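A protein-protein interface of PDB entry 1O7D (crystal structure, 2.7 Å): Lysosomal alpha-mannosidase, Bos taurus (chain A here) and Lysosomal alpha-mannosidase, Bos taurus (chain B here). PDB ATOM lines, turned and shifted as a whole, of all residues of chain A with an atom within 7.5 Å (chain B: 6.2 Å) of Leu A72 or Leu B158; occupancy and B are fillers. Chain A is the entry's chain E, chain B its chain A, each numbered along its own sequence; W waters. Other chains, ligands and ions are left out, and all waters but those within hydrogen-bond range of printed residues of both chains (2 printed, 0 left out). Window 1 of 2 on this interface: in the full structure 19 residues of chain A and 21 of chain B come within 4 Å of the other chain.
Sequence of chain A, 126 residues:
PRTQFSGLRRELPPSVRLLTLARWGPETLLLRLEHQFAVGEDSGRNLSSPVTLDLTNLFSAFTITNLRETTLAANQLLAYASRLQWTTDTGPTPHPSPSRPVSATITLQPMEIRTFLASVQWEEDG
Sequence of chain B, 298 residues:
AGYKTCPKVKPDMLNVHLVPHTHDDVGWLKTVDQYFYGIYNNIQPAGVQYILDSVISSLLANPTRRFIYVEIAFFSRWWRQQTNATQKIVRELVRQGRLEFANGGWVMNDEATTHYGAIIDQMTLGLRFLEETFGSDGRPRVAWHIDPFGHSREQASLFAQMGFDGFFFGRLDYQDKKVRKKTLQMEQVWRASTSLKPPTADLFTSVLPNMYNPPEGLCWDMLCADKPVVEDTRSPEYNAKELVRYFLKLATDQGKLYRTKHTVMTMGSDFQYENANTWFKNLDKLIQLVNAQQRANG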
ATOM      1  N   LEU A  19     -13.328  17.544 -13.019  1.00  0.00           N
ATOM      2  CA  LEU A  19     -13.469  18.951 -13.338  1.00  0.00           C
ATOM      3  C   LEU A  19     -12.515  19.823 -12.543  1.00  0.00           C
ATOM      4  O   LEU A  19     -11.770  20.620 -13.110  1.00  0.00           O
ATOM      5  CB  LEU A  19     -14.901  19.406 -13.084  1.00  0.00           C
ATOM      6  CG  LEU A  19     -15.176  20.854 -13.473  1.00  0.00           C
ATOM      7  CD1 LEU A  19     -14.577  21.158 -14.840  1.00  0.00           C
ATOM      8  CD2 LEU A  19     -16.669  21.092 -13.471  1.00  0.00           C
ATOM      9  N   LEU A  30     -10.954  21.377  -2.982  1.00  0.00           N
ATOM     10  CA  LEU A  30     -12.188  21.614  -3.716  1.00  0.00           C
ATOM     11  C   LEU A  30     -12.217  20.587  -4.831  1.00  0.00           C
ATOM     12  O   LEU A  30     -11.277  20.481  -5.609  1.00  0.00           O
ATOM     13  CB  LEU A  30     -12.219  23.025  -4.312  1.00  0.00           C
ATOM     14  CG  LEU A  30     -13.336  23.278  -5.344  1.00  0.00           C
ATOM     15  CD1 LEU A  30     -14.663  22.829  -4.786  1.00  0.00           C
ATOM     16  CD2 LEU A  30     -13.404  24.743  -5.721  1.00  0.00           C
ATOM     17  N   ARG A  32     -14.617  18.716  -8.026  1.00  0.00           N
ATOM     18  CA  ARG A  32     -15.801  18.710  -8.857  1.00  0.00           C
ATOM     19  C   ARG A  32     -15.663  17.559  -9.831  1.00  0.00           C
ATOM     20  O   ARG A  32     -14.599  17.336 -10.388  1.00  0.00           O
ATOM     21  CB  ARG A  32     -15.948  20.028  -9.611  1.00  0.00           C
ATOM     22  CG  ARG A  32     -16.372  21.210  -8.740  1.00  0.00           C
ATOM     23  CD  ARG A  32     -17.048  22.290  -9.586  1.00  0.00           C
ATOM     24  NE  ARG A  32     -17.283  23.544  -8.867  1.00  0.00           N
ATOM     25  CZ  ARG A  32     -16.412  24.552  -8.778  1.00  0.00           C
ATOM     26  NH1 ARG A  32     -15.225  24.475  -9.363  1.00  0.00           N
ATOM     27  NH2 ARG A  32     -16.735  25.654  -8.116  1.00  0.00           N
ATOM     28  N   THR A  70     -22.081  20.561  -2.092  1.00  0.00           N
ATOM     29  CA  THR A  70     -22.173  21.976  -2.373  1.00  0.00           C
ATOM     30  C   THR A  70     -22.807  22.363  -3.725  1.00  0.00           C
ATOM     31  O   THR A  70     -22.998  21.521  -4.613  1.00  0.00           O
ATOM     32  CB  THR A  70     -20.742  22.579  -2.211  1.00  0.00           C
ATOM     33  OG1 THR A  70     -20.737  23.507  -1.122  1.00  0.00           O
ATOM     34  CG2 THR A  70     -20.263  23.258  -3.479  1.00  0.00           C
ATOM     35  N   THR A  71     -23.160  23.643  -3.847  1.00  0.00           N
ATOM     36  CA  THR A  71     -23.743  24.186  -5.067  1.00  0.00           C
ATOM     37  C   THR A  71     -22.563  24.436  -6.000  1.00  0.00           C
ATOM     38  O   THR A  71     -21.436  24.599  -5.541  1.00  0.00           O
ATOM     39  CB  THR A  71     -24.503  25.519  -4.792  1.00  0.00           C
ATOM     40  OG1 THR A  71     -23.578  26.571  -4.491  1.00  0.00           O
ATOM     41  CG2 THR A  71     -25.417  25.357  -3.605  1.00  0.00           C
ATOM     42  N   LEU A  72     -22.813  24.483  -7.299  1.00  0.00           N
ATOM     43  CA  LEU A  72     -21.723  24.662  -8.250  1.00  0.00           C
ATOM     44  C   LEU A  72     -20.620  25.677  -7.907  1.00  0.00           C
ATOM     45  O   LEU A  72     -19.447  25.345  -8.002  1.00  0.00           O
ATOM     46  CB  LEU A  72     -22.288  24.951  -9.642  1.00  0.00           C
ATOM     47  CG  LEU A  72     -21.318  24.896 -10.821  1.00  0.00           C
ATOM     48  CD1 LEU A  72     -20.549  23.583 -10.848  1.00  0.00           C
ATOM     49  CD2 LEU A  72     -22.118  25.083 -12.103  1.00  0.00           C
ATOM     50  N   ALA A  73     -20.974  26.893  -7.501  1.00  0.00           N
ATOM     51  CA  ALA A  73     -19.953  27.896  -7.197  1.00  0.00           C
ATOM     52  C   ALA A  73     -19.372  27.762  -5.803  1.00  0.00           C
ATOM     53  O   ALA A  73     -18.659  28.642  -5.338  1.00  0.00           O
ATOM     54  CB  ALA A  73     -20.498  29.288  -7.387  1.00  0.00           C
ATOM     55  N   ALA A  74     -19.713  26.670  -5.136  1.00  0.00           N
ATOM     56  CA  ALA A  74     -19.205  26.397  -3.817  1.00  0.00           C
ATOM     57  C   ALA A  74     -19.483  27.478  -2.759  1.00  0.00           C
ATOM     58  O   ALA A  74     -18.681  27.667  -1.850  1.00  0.00           O
ATOM     59  CB  ALA A  74     -17.685  26.137  -3.916  1.00  0.00           C
ATOM     60  N   ASN A  75     -20.612  28.171  -2.833  1.00  0.00           N
ATOM     61  CA  ASN A  75     -20.876  29.190  -1.833  1.00  0.00           C
ATOM     62  C   ASN A  75     -22.023  28.884  -0.875  1.00  0.00           C
ATOM     63  O   ASN A  75     -22.305  29.687   0.016  1.00  0.00           O
ATOM     64  CB  ASN A  75     -21.075  30.559  -2.503  1.00  0.00           C
ATOM     65  CG  ASN A  75     -22.206  30.568  -3.518  1.00  0.00           C
ATOM     66  OD1 ASN A  75     -22.465  29.566  -4.186  1.00  0.00           O
ATOM     67  ND2 ASN A  75     -22.873  31.710  -3.649  1.00  0.00           N
ATOM     68  N   GLN A  76     -22.676  27.730  -1.059  1.00  0.00           N
ATOM     69  CA  GLN A  76     -23.782  27.274  -0.192  1.00  0.00           C
ATOM     70  C   GLN A  76     -23.669  25.765   0.026  1.00  0.00           C
ATOM     71  O   GLN A  76     -23.035  25.052  -0.760  1.00  0.00           O
ATOM     72  CB  GLN A  76     -25.160  27.499  -0.826  1.00  0.00           C
ATOM     73  CG  GLN A  76     -25.541  28.896  -1.195  1.00  0.00           C
ATOM     74  CD  GLN A  76     -27.009  28.984  -1.598  1.00  0.00           C
ATOM     75  OE1 GLN A  76     -27.909  28.842  -0.762  1.00  0.00           O
ATOM     76  NE2 GLN A  76     -27.257  29.208  -2.886  1.00  0.00           N
ATOM     77  N   LEU A  78     -25.283  22.547  -0.463  1.00  0.00           N
ATOM     78  CA  LEU A  78     -26.353  21.969  -1.264  1.00  0.00           C
ATOM     79  C   LEU A  78     -27.576  21.490  -0.477  1.00  0.00           C
ATOM     80  O   LEU A  78     -28.708  21.679  -0.924  1.00  0.00           O
ATOM     81  CB  LEU A  78     -25.810  20.808  -2.095  1.00  0.00           C
ATOM     82  CG  LEU A  78     -26.786  20.230  -3.118  1.00  0.00           C
ATOM     83  CD1 LEU A  78     -27.146  21.299  -4.120  1.00  0.00           C
ATOM     84  CD2 LEU A  78     -26.153  19.044  -3.823  1.00  0.00           C
ATOM     85  N   ILE A 113     -22.912  17.828 -12.618  1.00  0.00           N
ATOM     86  CA  ILE A 113     -21.649  18.234 -12.007  1.00  0.00           C
ATOM     87  C   ILE A 113     -21.869  18.340 -10.508  1.00  0.00           C
ATOM     88  O   ILE A 113     -22.718  19.107 -10.056  1.00  0.00           O
ATOM     89  CB  ILE A 113     -21.196  19.630 -12.467  1.00  0.00           C
ATOM     90  CG1 ILE A 113     -20.914  19.634 -13.970  1.00  0.00           C
ATOM     91  CG2 ILE A 113     -19.980  20.059 -11.654  1.00  0.00           C
ATOM     92  CD1 ILE A 113     -20.633  21.018 -14.543  1.00  0.00           C
ATOM     93  N   ARG A 114     -21.117  17.584  -9.728  1.00  0.00           N
ATOM     94  CA  ARG A 114     -21.274  17.675  -8.290  1.00  0.00           C
ATOM     95  C   ARG A 114     -20.022  18.291  -7.660  1.00  0.00           C
ATOM     96  O   ARG A 114     -18.888  17.939  -8.009  1.00  0.00           O
ATOM     97  CB  ARG A 114     -21.609  16.294  -7.713  1.00  0.00           C
ATOM     98  CG  ARG A 114     -22.964  15.798  -8.205  1.00  0.00           C
ATOM     99  CD  ARG A 114     -23.312  14.442  -7.669  1.00  0.00           C
ATOM    100  NE  ARG A 114     -23.301  14.423  -6.212  1.00  0.00           N
ATOM    101  CZ  ARG A 114     -23.821  13.440  -5.481  1.00  0.00           C
ATOM    102  NH1 ARG A 114     -24.395  12.395  -6.072  1.00  0.00           N
ATOM    103  NH2 ARG A 114     -23.763  13.502  -4.157  1.00  0.00           N
ATOM    104  N   THR A 115     -20.246  19.230  -6.744  1.00  0.00           N
ATOM    105  CA  THR A 115     -19.164  19.952  -6.075  1.00  0.00           C
ATOM    106  C   THR A 115     -18.999  19.572  -4.602  1.00  0.00           C
ATOM    107  O   THR A 115     -19.963  19.553  -3.834  1.00  0.00           O
ATOM    108  CB  THR A 115     -19.405  21.475  -6.178  1.00  0.00           C
ATOM    109  OG1 THR A 115     -19.883  21.790  -7.492  1.00  0.00           O
ATOM    110  CG2 THR A 115     -18.113  22.237  -5.922  1.00  0.00           C
ATOM    111  N   PHE A 116     -17.758  19.300  -4.209  1.00  0.00           N
ATOM    112  CA  PHE A 116     -17.457  18.899  -2.838  1.00  0.00           C
ATOM    113  C   PHE A 116     -16.316  19.643  -2.183  1.00  0.00           C
ATOM    114  O   PHE A 116     -15.355  20.030  -2.838  1.00  0.00           O
ATOM    115  CB  PHE A 116     -17.113  17.408  -2.785  1.00  0.00           C
ATOM    116  CG  PHE A 116     -18.172  16.521  -3.359  1.00  0.00           C
ATOM    117  CD1 PHE A 116     -18.246  16.310  -4.733  1.00  0.00           C
ATOM    118  CD2 PHE A 116     -19.135  15.947  -2.538  1.00  0.00           C
ATOM    119  CE1 PHE A 116     -19.264  15.543  -5.287  1.00  0.00           C
ATOM    120  CE2 PHE A 116     -20.156  15.179  -3.074  1.00  0.00           C
ATOM    121  CZ  PHE A 116     -20.224  14.976  -4.459  1.00  0.00           C
ATOM    122  N   HIS B 115     -15.276  29.436 -21.757  1.00  0.00           N
ATOM    123  CA  HIS B 115     -15.293  27.996 -21.535  1.00  0.00           C
ATOM    124  C   HIS B 115     -16.122  27.782 -20.285  1.00  0.00           C
ATOM    125  O   HIS B 115     -15.898  28.472 -19.302  1.00  0.00           O
ATOM    126  CB  HIS B 115     -13.855  27.521 -21.302  1.00  0.00           C
ATOM    127  CG  HIS B 115     -13.742  26.076 -20.935  1.00  0.00           C
ATOM    128  ND1 HIS B 115     -14.120  25.059 -21.781  1.00  0.00           N
ATOM    129  CD2 HIS B 115     -13.296  25.483 -19.806  1.00  0.00           C
ATOM    130  CE1 HIS B 115     -13.914  23.897 -21.190  1.00  0.00           C
ATOM    131  NE2 HIS B 115     -13.413  24.126 -19.992  1.00  0.00           N
ATOM    132  N   TYR B 116     -17.061  26.839 -20.292  1.00  0.00           N
ATOM    133  CA  TYR B 116     -17.897  26.637 -19.105  1.00  0.00           C
ATOM    134  C   TYR B 116     -17.093  26.501 -17.799  1.00  0.00           C
ATOM    135  O   TYR B 116     -17.495  27.011 -16.754  1.00  0.00           O
ATOM    136  CB  TYR B 116     -18.804  25.418 -19.298  1.00  0.00           C
ATOM    137  CG  TYR B 116     -18.144  24.099 -19.013  1.00  0.00           C
ATOM    138  CD1 TYR B 116     -18.050  23.606 -17.709  1.00  0.00           C
ATOM    139  CD2 TYR B 116     -17.575  23.361 -20.033  1.00  0.00           C
ATOM    140  CE1 TYR B 116     -17.395  22.408 -17.435  1.00  0.00           C
ATOM    141  CE2 TYR B 116     -16.921  22.168 -19.776  1.00  0.00           C
ATOM    142  CZ  TYR B 116     -16.826  21.690 -18.479  1.00  0.00           C
ATOM    143  OH  TYR B 116     -16.145  20.502 -18.241  1.00  0.00           O
ATOM    144  N   GLY B 117     -15.947  25.830 -17.872  1.00  0.00           N
ATOM    145  CA  GLY B 117     -15.126  25.629 -16.695  1.00  0.00           C
ATOM    146  C   GLY B 117     -14.517  26.910 -16.189  1.00  0.00           C
ATOM    147  O   GLY B 117     -14.388  27.108 -14.993  1.00  0.00           O
ATOM    148  N   ILE B 119     -15.794  29.903 -16.680  1.00  0.00           N
ATOM    149  CA  ILE B 119     -16.883  30.728 -16.186  1.00  0.00           C
ATOM    150  C   ILE B 119     -17.134  30.385 -14.720  1.00  0.00           C
ATOM    151  O   ILE B 119     -17.470  31.240 -13.914  1.00  0.00           O
ATOM    152  CB  ILE B 119     -18.168  30.457 -16.990  1.00  0.00           C
ATOM    153  CG1 ILE B 119     -17.989  30.965 -18.417  1.00  0.00           C
ATOM    154  CG2 ILE B 119     -19.369  31.114 -16.326  1.00  0.00           C
ATOM    155  CD1 ILE B 119     -19.061  30.468 -19.371  1.00  0.00           C
ATOM    156  N   ILE B 120     -16.970  29.119 -14.377  1.00  0.00           N
ATOM    157  CA  ILE B 120     -17.187  28.690 -13.009  1.00  0.00           C
ATOM    158  C   ILE B 120     -16.095  29.208 -12.068  1.00  0.00           C
ATOM    159  O   ILE B 120     -16.394  29.745 -10.999  1.00  0.00           O
ATOM    160  CB  ILE B 120     -17.264  27.159 -12.937  1.00  0.00           C
ATOM    161  CG1 ILE B 120     -18.370  26.668 -13.874  1.00  0.00           C
ATOM    162  CG2 ILE B 120     -17.532  26.708 -11.507  1.00  0.00           C
ATOM    163  CD1 ILE B 120     -18.482  25.150 -13.944  1.00  0.00           C
ATOM    164  N   THR B 124     -17.158  31.382  -8.902  1.00  0.00           N
ATOM    165  CA  THR B 124     -16.773  30.904  -7.579  1.00  0.00           C
ATOM    166  C   THR B 124     -15.910  31.940  -6.885  1.00  0.00           C
ATOM    167  O   THR B 124     -15.999  32.131  -5.685  1.00  0.00           O
ATOM    168  CB  THR B 124     -15.930  29.613  -7.670  1.00  0.00           C
ATOM    169  OG1 THR B 124     -16.740  28.527  -8.133  1.00  0.00           O
ATOM    170  CG2 THR B 124     -15.333  29.271  -6.324  1.00  0.00           C
ATOM    171  N   ARG B 153     -27.228  28.912 -23.931  1.00  0.00           N
ATOM    172  CA  ARG B 153     -28.060  28.073 -23.097  1.00  0.00           C
ATOM    173  C   ARG B 153     -27.255  27.506 -21.924  1.00  0.00           C
ATOM    174  O   ARG B 153     -27.799  27.289 -20.839  1.00  0.00           O
ATOM    175  CB  ARG B 153     -28.671  26.931 -23.903  1.00  0.00           C
ATOM    176  CG  ARG B 153     -29.835  26.311 -23.173  1.00  0.00           C
ATOM    177  CD  ARG B 153     -30.439  25.163 -23.926  1.00  0.00           C
ATOM    178  NE  ARG B 153     -29.530  24.026 -24.014  1.00  0.00           N
ATOM    179  CZ  ARG B 153     -29.748  22.956 -24.775  1.00  0.00           C
ATOM    180  NH1 ARG B 153     -30.847  22.882 -25.518  1.00  0.00           N
ATOM    181  NH2 ARG B 153     -28.870  21.956 -24.796  1.00  0.00           N
ATOM    182  N   GLU B 154     -25.956  27.283 -22.122  1.00  0.00           N
ATOM    183  CA  GLU B 154     -25.143  26.731 -21.047  1.00  0.00           C
ATOM    184  C   GLU B 154     -25.072  27.702 -19.861  1.00  0.00           C
ATOM    185  O   GLU B 154     -25.188  27.290 -18.702  1.00  0.00           O
ATOM    186  CB  GLU B 154     -23.746  26.395 -21.556  1.00  0.00           C
ATOM    187  CG  GLU B 154     -23.029  25.382 -20.683  1.00  0.00           C
ATOM    188  CD  GLU B 154     -23.795  24.051 -20.576  1.00  0.00           C
ATOM    189  OE1 GLU B 154     -24.086  23.438 -21.624  1.00  0.00           O
ATOM    190  OE2 GLU B 154     -24.110  23.599 -19.451  1.00  0.00           O
ATOM    191  N   GLN B 155     -24.893  28.990 -20.149  1.00  0.00           N
ATOM    192  CA  GLN B 155     -24.856  29.998 -19.097  1.00  0.00           C
ATOM    193  C   GLN B 155     -26.075  29.825 -18.177  1.00  0.00           C
ATOM    194  O   GLN B 155     -25.947  29.777 -16.958  1.00  0.00           O
ATOM    195  CB  GLN B 155     -24.885  31.397 -19.714  1.00  0.00           C
ATOM    196  CG  GLN B 155     -24.688  32.536 -18.723  1.00  0.00           C
ATOM    197  CD  GLN B 155     -23.347  32.448 -18.011  1.00  0.00           C
ATOM    198  OE1 GLN B 155     -22.965  33.335 -17.234  1.00  0.00           O
ATOM    199  NE2 GLN B 155     -22.624  31.366 -18.270  1.00  0.00           N
ATOM    200  N   ALA B 156     -27.259  29.728 -18.771  1.00  0.00           N
ATOM    201  CA  ALA B 156     -28.475  29.572 -17.992  1.00  0.00           C
ATOM    202  C   ALA B 156     -28.394  28.316 -17.137  1.00  0.00           C
ATOM    203  O   ALA B 156     -28.779  28.319 -15.971  1.00  0.00           O
ATOM    204  CB  ALA B 156     -29.672  29.515 -18.916  1.00  0.00           C
ATOM    205  N   SER B 157     -27.887  27.243 -17.732  1.00  0.00           N
ATOM    206  CA  SER B 157     -27.710  25.968 -17.032  1.00  0.00           C
ATOM    207  C   SER B 157     -26.777  26.144 -15.828  1.00  0.00           C
ATOM    208  O   SER B 157     -27.061  25.655 -14.746  1.00  0.00           O
ATOM    209  CB  SER B 157     -27.109  24.924 -17.985  1.00  0.00           C
ATOM    210  OG  SER B 157     -26.694  23.753 -17.297  1.00  0.00           O
ATOM    211  N   LEU B 158     -25.664  26.841 -16.040  1.00  0.00           N
ATOM    212  CA  LEU B 158     -24.683  27.090 -14.997  1.00  0.00           C
ATOM    213  C   LEU B 158     -25.260  27.891 -13.847  1.00  0.00           C
ATOM    214  O   LEU B 158     -25.072  27.532 -12.679  1.00  0.00           O
ATOM    215  CB  LEU B 158     -23.465  27.812 -15.585  1.00  0.00           C
ATOM    216  CG  LEU B 158     -22.223  26.983 -15.965  1.00  0.00           C
ATOM    217  CD1 LEU B 158     -22.582  25.600 -16.490  1.00  0.00           C
ATOM    218  CD2 LEU B 158     -21.443  27.756 -16.994  1.00  0.00           C
ATOM    219  N   PHE B 159     -25.955  28.981 -14.163  1.00  0.00           N
ATOM    220  CA  PHE B 159     -26.555  29.784 -13.104  1.00  0.00           C
ATOM    221  C   PHE B 159     -27.619  28.969 -12.354  1.00  0.00           C
ATOM    222  O   PHE B 159     -27.667  28.979 -11.130  1.00  0.00           O
ATOM    223  CB  PHE B 159     -27.178  31.062 -13.667  1.00  0.00           C
ATOM    224  CG  PHE B 159     -26.177  32.132 -14.025  1.00  0.00           C
ATOM    225  CD1 PHE B 159     -25.055  32.351 -13.239  1.00  0.00           C
ATOM    226  CD2 PHE B 159     -26.400  32.970 -15.116  1.00  0.00           C
ATOM    227  CE1 PHE B 159     -24.160  33.391 -13.531  1.00  0.00           C
ATOM    228  CE2 PHE B 159     -25.511  34.016 -15.417  1.00  0.00           C
ATOM    229  CZ  PHE B 159     -24.389  34.225 -14.616  1.00  0.00           C
ATOM    230  N   ALA B 160     -28.471  28.259 -13.083  1.00  0.00           N
ATOM    231  CA  ALA B 160     -29.486  27.439 -12.440  1.00  0.00           C
ATOM    232  C   ALA B 160     -28.835  26.486 -11.442  1.00  0.00           C
ATOM    233  O   ALA B 160     -29.322  26.334 -10.321  1.00  0.00           O
ATOM    234  CB  ALA B 160     -30.249  26.651 -13.474  1.00  0.00           C
ATOM    235  N   GLN B 161     -27.737  25.849 -11.853  1.00  0.00           N
ATOM    236  CA  GLN B 161     -27.017  24.895 -11.002  1.00  0.00           C
ATOM    237  C   GLN B 161     -26.285  25.568  -9.853  1.00  0.00           C
ATOM    238  O   GLN B 161     -25.811  24.888  -8.954  1.00  0.00           O
ATOM    239  CB  GLN B 161     -25.980  24.095 -11.797  1.00  0.00           C
ATOM    240  CG  GLN B 161     -26.499  23.212 -12.920  1.00  0.00           C
ATOM    241  CD  GLN B 161     -25.362  22.517 -13.668  1.00  0.00           C
ATOM    242  OE1 GLN B 161     -24.602  21.735 -13.088  1.00  0.00           O
ATOM    243  NE2 GLN B 161     -25.233  22.813 -14.957  1.00  0.00           N
ATOM    244  N   MET B 162     -26.147  26.891  -9.891  1.00  0.00           N
ATOM    245  CA  MET B 162     -25.471  27.589  -8.807  1.00  0.00           C
ATOM    246  C   MET B 162     -26.489  28.052  -7.764  1.00  0.00           C
ATOM    247  O   MET B 162     -26.122  28.590  -6.713  1.00  0.00           O
ATOM    248  CB  MET B 162     -24.675  28.776  -9.350  1.00  0.00           C
ATOM    249  CG  MET B 162     -23.419  28.375 -10.104  1.00  0.00           C
ATOM    250  SD  MET B 162     -22.426  29.755 -10.772  1.00  0.00           S
ATOM    251  CE  MET B 162     -22.723  29.553 -12.506  1.00  0.00           C
ATOM    252  N   GLY B 163     -27.771  27.835  -8.056  1.00  0.00           N
ATOM    253  CA  GLY B 163     -28.828  28.215  -7.132  1.00  0.00           C
ATOM    254  C   GLY B 163     -29.427  29.601  -7.293  1.00  0.00           C
ATOM    255  O   GLY B 163     -29.996  30.159  -6.350  1.00  0.00           O
ATOM    256  N   PHE B 164     -29.291  30.173  -8.479  1.00  0.00           N
ATOM    257  CA  PHE B 164     -29.853  31.488  -8.740  1.00  0.00           C
ATOM    258  C   PHE B 164     -31.324  31.268  -9.087  1.00  0.00           C
ATOM    259  O   PHE B 164     -31.660  30.303  -9.763  1.00  0.00           O
ATOM    260  CB  PHE B 164     -29.132  32.147  -9.925  1.00  0.00           C
ATOM    261  CG  PHE B 164     -27.817  32.801  -9.576  1.00  0.00           C
ATOM    262  CD1 PHE B 164     -27.774  33.892  -8.722  1.00  0.00           C
ATOM    263  CD2 PHE B 164     -26.632  32.355 -10.136  1.00  0.00           C
ATOM    264  CE1 PHE B 164     -26.567  34.535  -8.431  1.00  0.00           C
ATOM    265  CE2 PHE B 164     -25.426  32.990  -9.851  1.00  0.00           C
ATOM    266  CZ  PHE B 164     -25.395  34.084  -8.997  1.00  0.00           C
ATOM    267  N   ALA B 192     -32.566  25.252 -19.888  1.00  0.00           N
ATOM    268  CA  ALA B 192     -31.238  25.269 -20.471  1.00  0.00           C
ATOM    269  C   ALA B 192     -30.547  23.943 -20.649  1.00  0.00           C
ATOM    270  O   ALA B 192     -29.432  23.907 -21.145  1.00  0.00           O
ATOM    271  CB  ALA B 192     -30.346  26.193 -19.682  1.00  0.00           C
HETATM  272  O   HOH W   1     -28.486  32.182  -4.193  1.00  0.00           O
HETATM  273  O   HOH W   2     -17.374  30.717  -3.623  1.00  0.00           O
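Water W2 lies within hydrogen-bond range of the backbone carbonyl oxygen (O) of Thr B124 and the backbone carbonyl oxygen (O) of Ala A73.
Water W1 bridges the backbone carbonyl oxygen (O) of Gly B163 (3.3 Å) and the side-chain amide nitrogen (NE2) of Gln A76 (3.5 Å).
Of the 15 printed residues of chain A, 5 touch a printed residue of chain B.
Hydrophobic or aromatic side chains of chain A that line the printed part of chain B: Leu A19, Leu A72 and Ala A73.
Hydrophobic or aromatic side chains of chain B within 4 Å of the printed part of chain A: Tyr B116, Ile B120 and Met B162.
Among the printed residues, 9 pairs touch across the chains.
Among the printed residues, no Asp or Glu carboxylate lies within 4 Å of a Lys or Arg side-chain nitrogen of the other chain.
OG1 of Thr B124 is in hydrogen-bond range of NH2 of Arg A32 (2.9 Å).
OG1 of Thr B124 lies within hydrogen-bond range of O of Ala A73 (3.4 Å).
N of Leu A72 lies within hydrogen-bond range of O of Gln B161.
The side-chain hydroxyl of Thr B124 sits at hydrogen-bond distance from the backbone carbonyl oxygen of Ile B120 (3.1 Å).
OG of Ser B157 is in hydrogen-bond range of NE2 of Gln B161 (2.9 Å).
O of Arg A32 lies within hydrogen-bond range of N of Leu A19.
The backbone carbonyl oxygen (O) of Leu A72 lies within hydrogen-bond range of the guanidinium group (NH2) of Arg A32, 2.7 Å away.
OG1 of Thr A115 lies close to NE of Arg A32 (3.4 Å).
The backbone NH (N) of Thr A71 lies within hydrogen-bond range of the backbone carbonyl oxygen (O) of Gln A76, at 3.4 Å.
Leu A72 touches three residues of chain B.
Of chain A, only Leu A72 comes within 4 Å of Leu B158.
Of the printed residues of chain B, Arg A32 touches Ile B120 and Thr B124.
Of the printed residues of chain A, Met B162 touches Thr A71 (3.9 Å), Leu A72 (3.6 Å) and Ala A73 (3.9 Å).
Printed residues of chain B within 4 Å of Thr A71: Met B162.
Ser B157 touches none of the printed residues of chain A.
The nearest residue of chain B that does not touch Leu A72 is Ile B120 (4.04 Å).
The nearest residue of chain A that does not touch Leu B158 is Ile A113 (5.3 Å).
Leu A19 touches Tyr B116 (CD1 to OH, 3.8 Å).
NH2 of Arg A32 touches CG2 of Ile B120, 3.6 Å away.
O of Met B162 touches OG1 of Thr A71 (3.9 Å).
CD2 of Leu A72 touches O of Leu B158, 3.9 Å away.
Leu A72 touches Met B162.
N of Ala A73 touches CG of Met B162 (3.9 Å).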
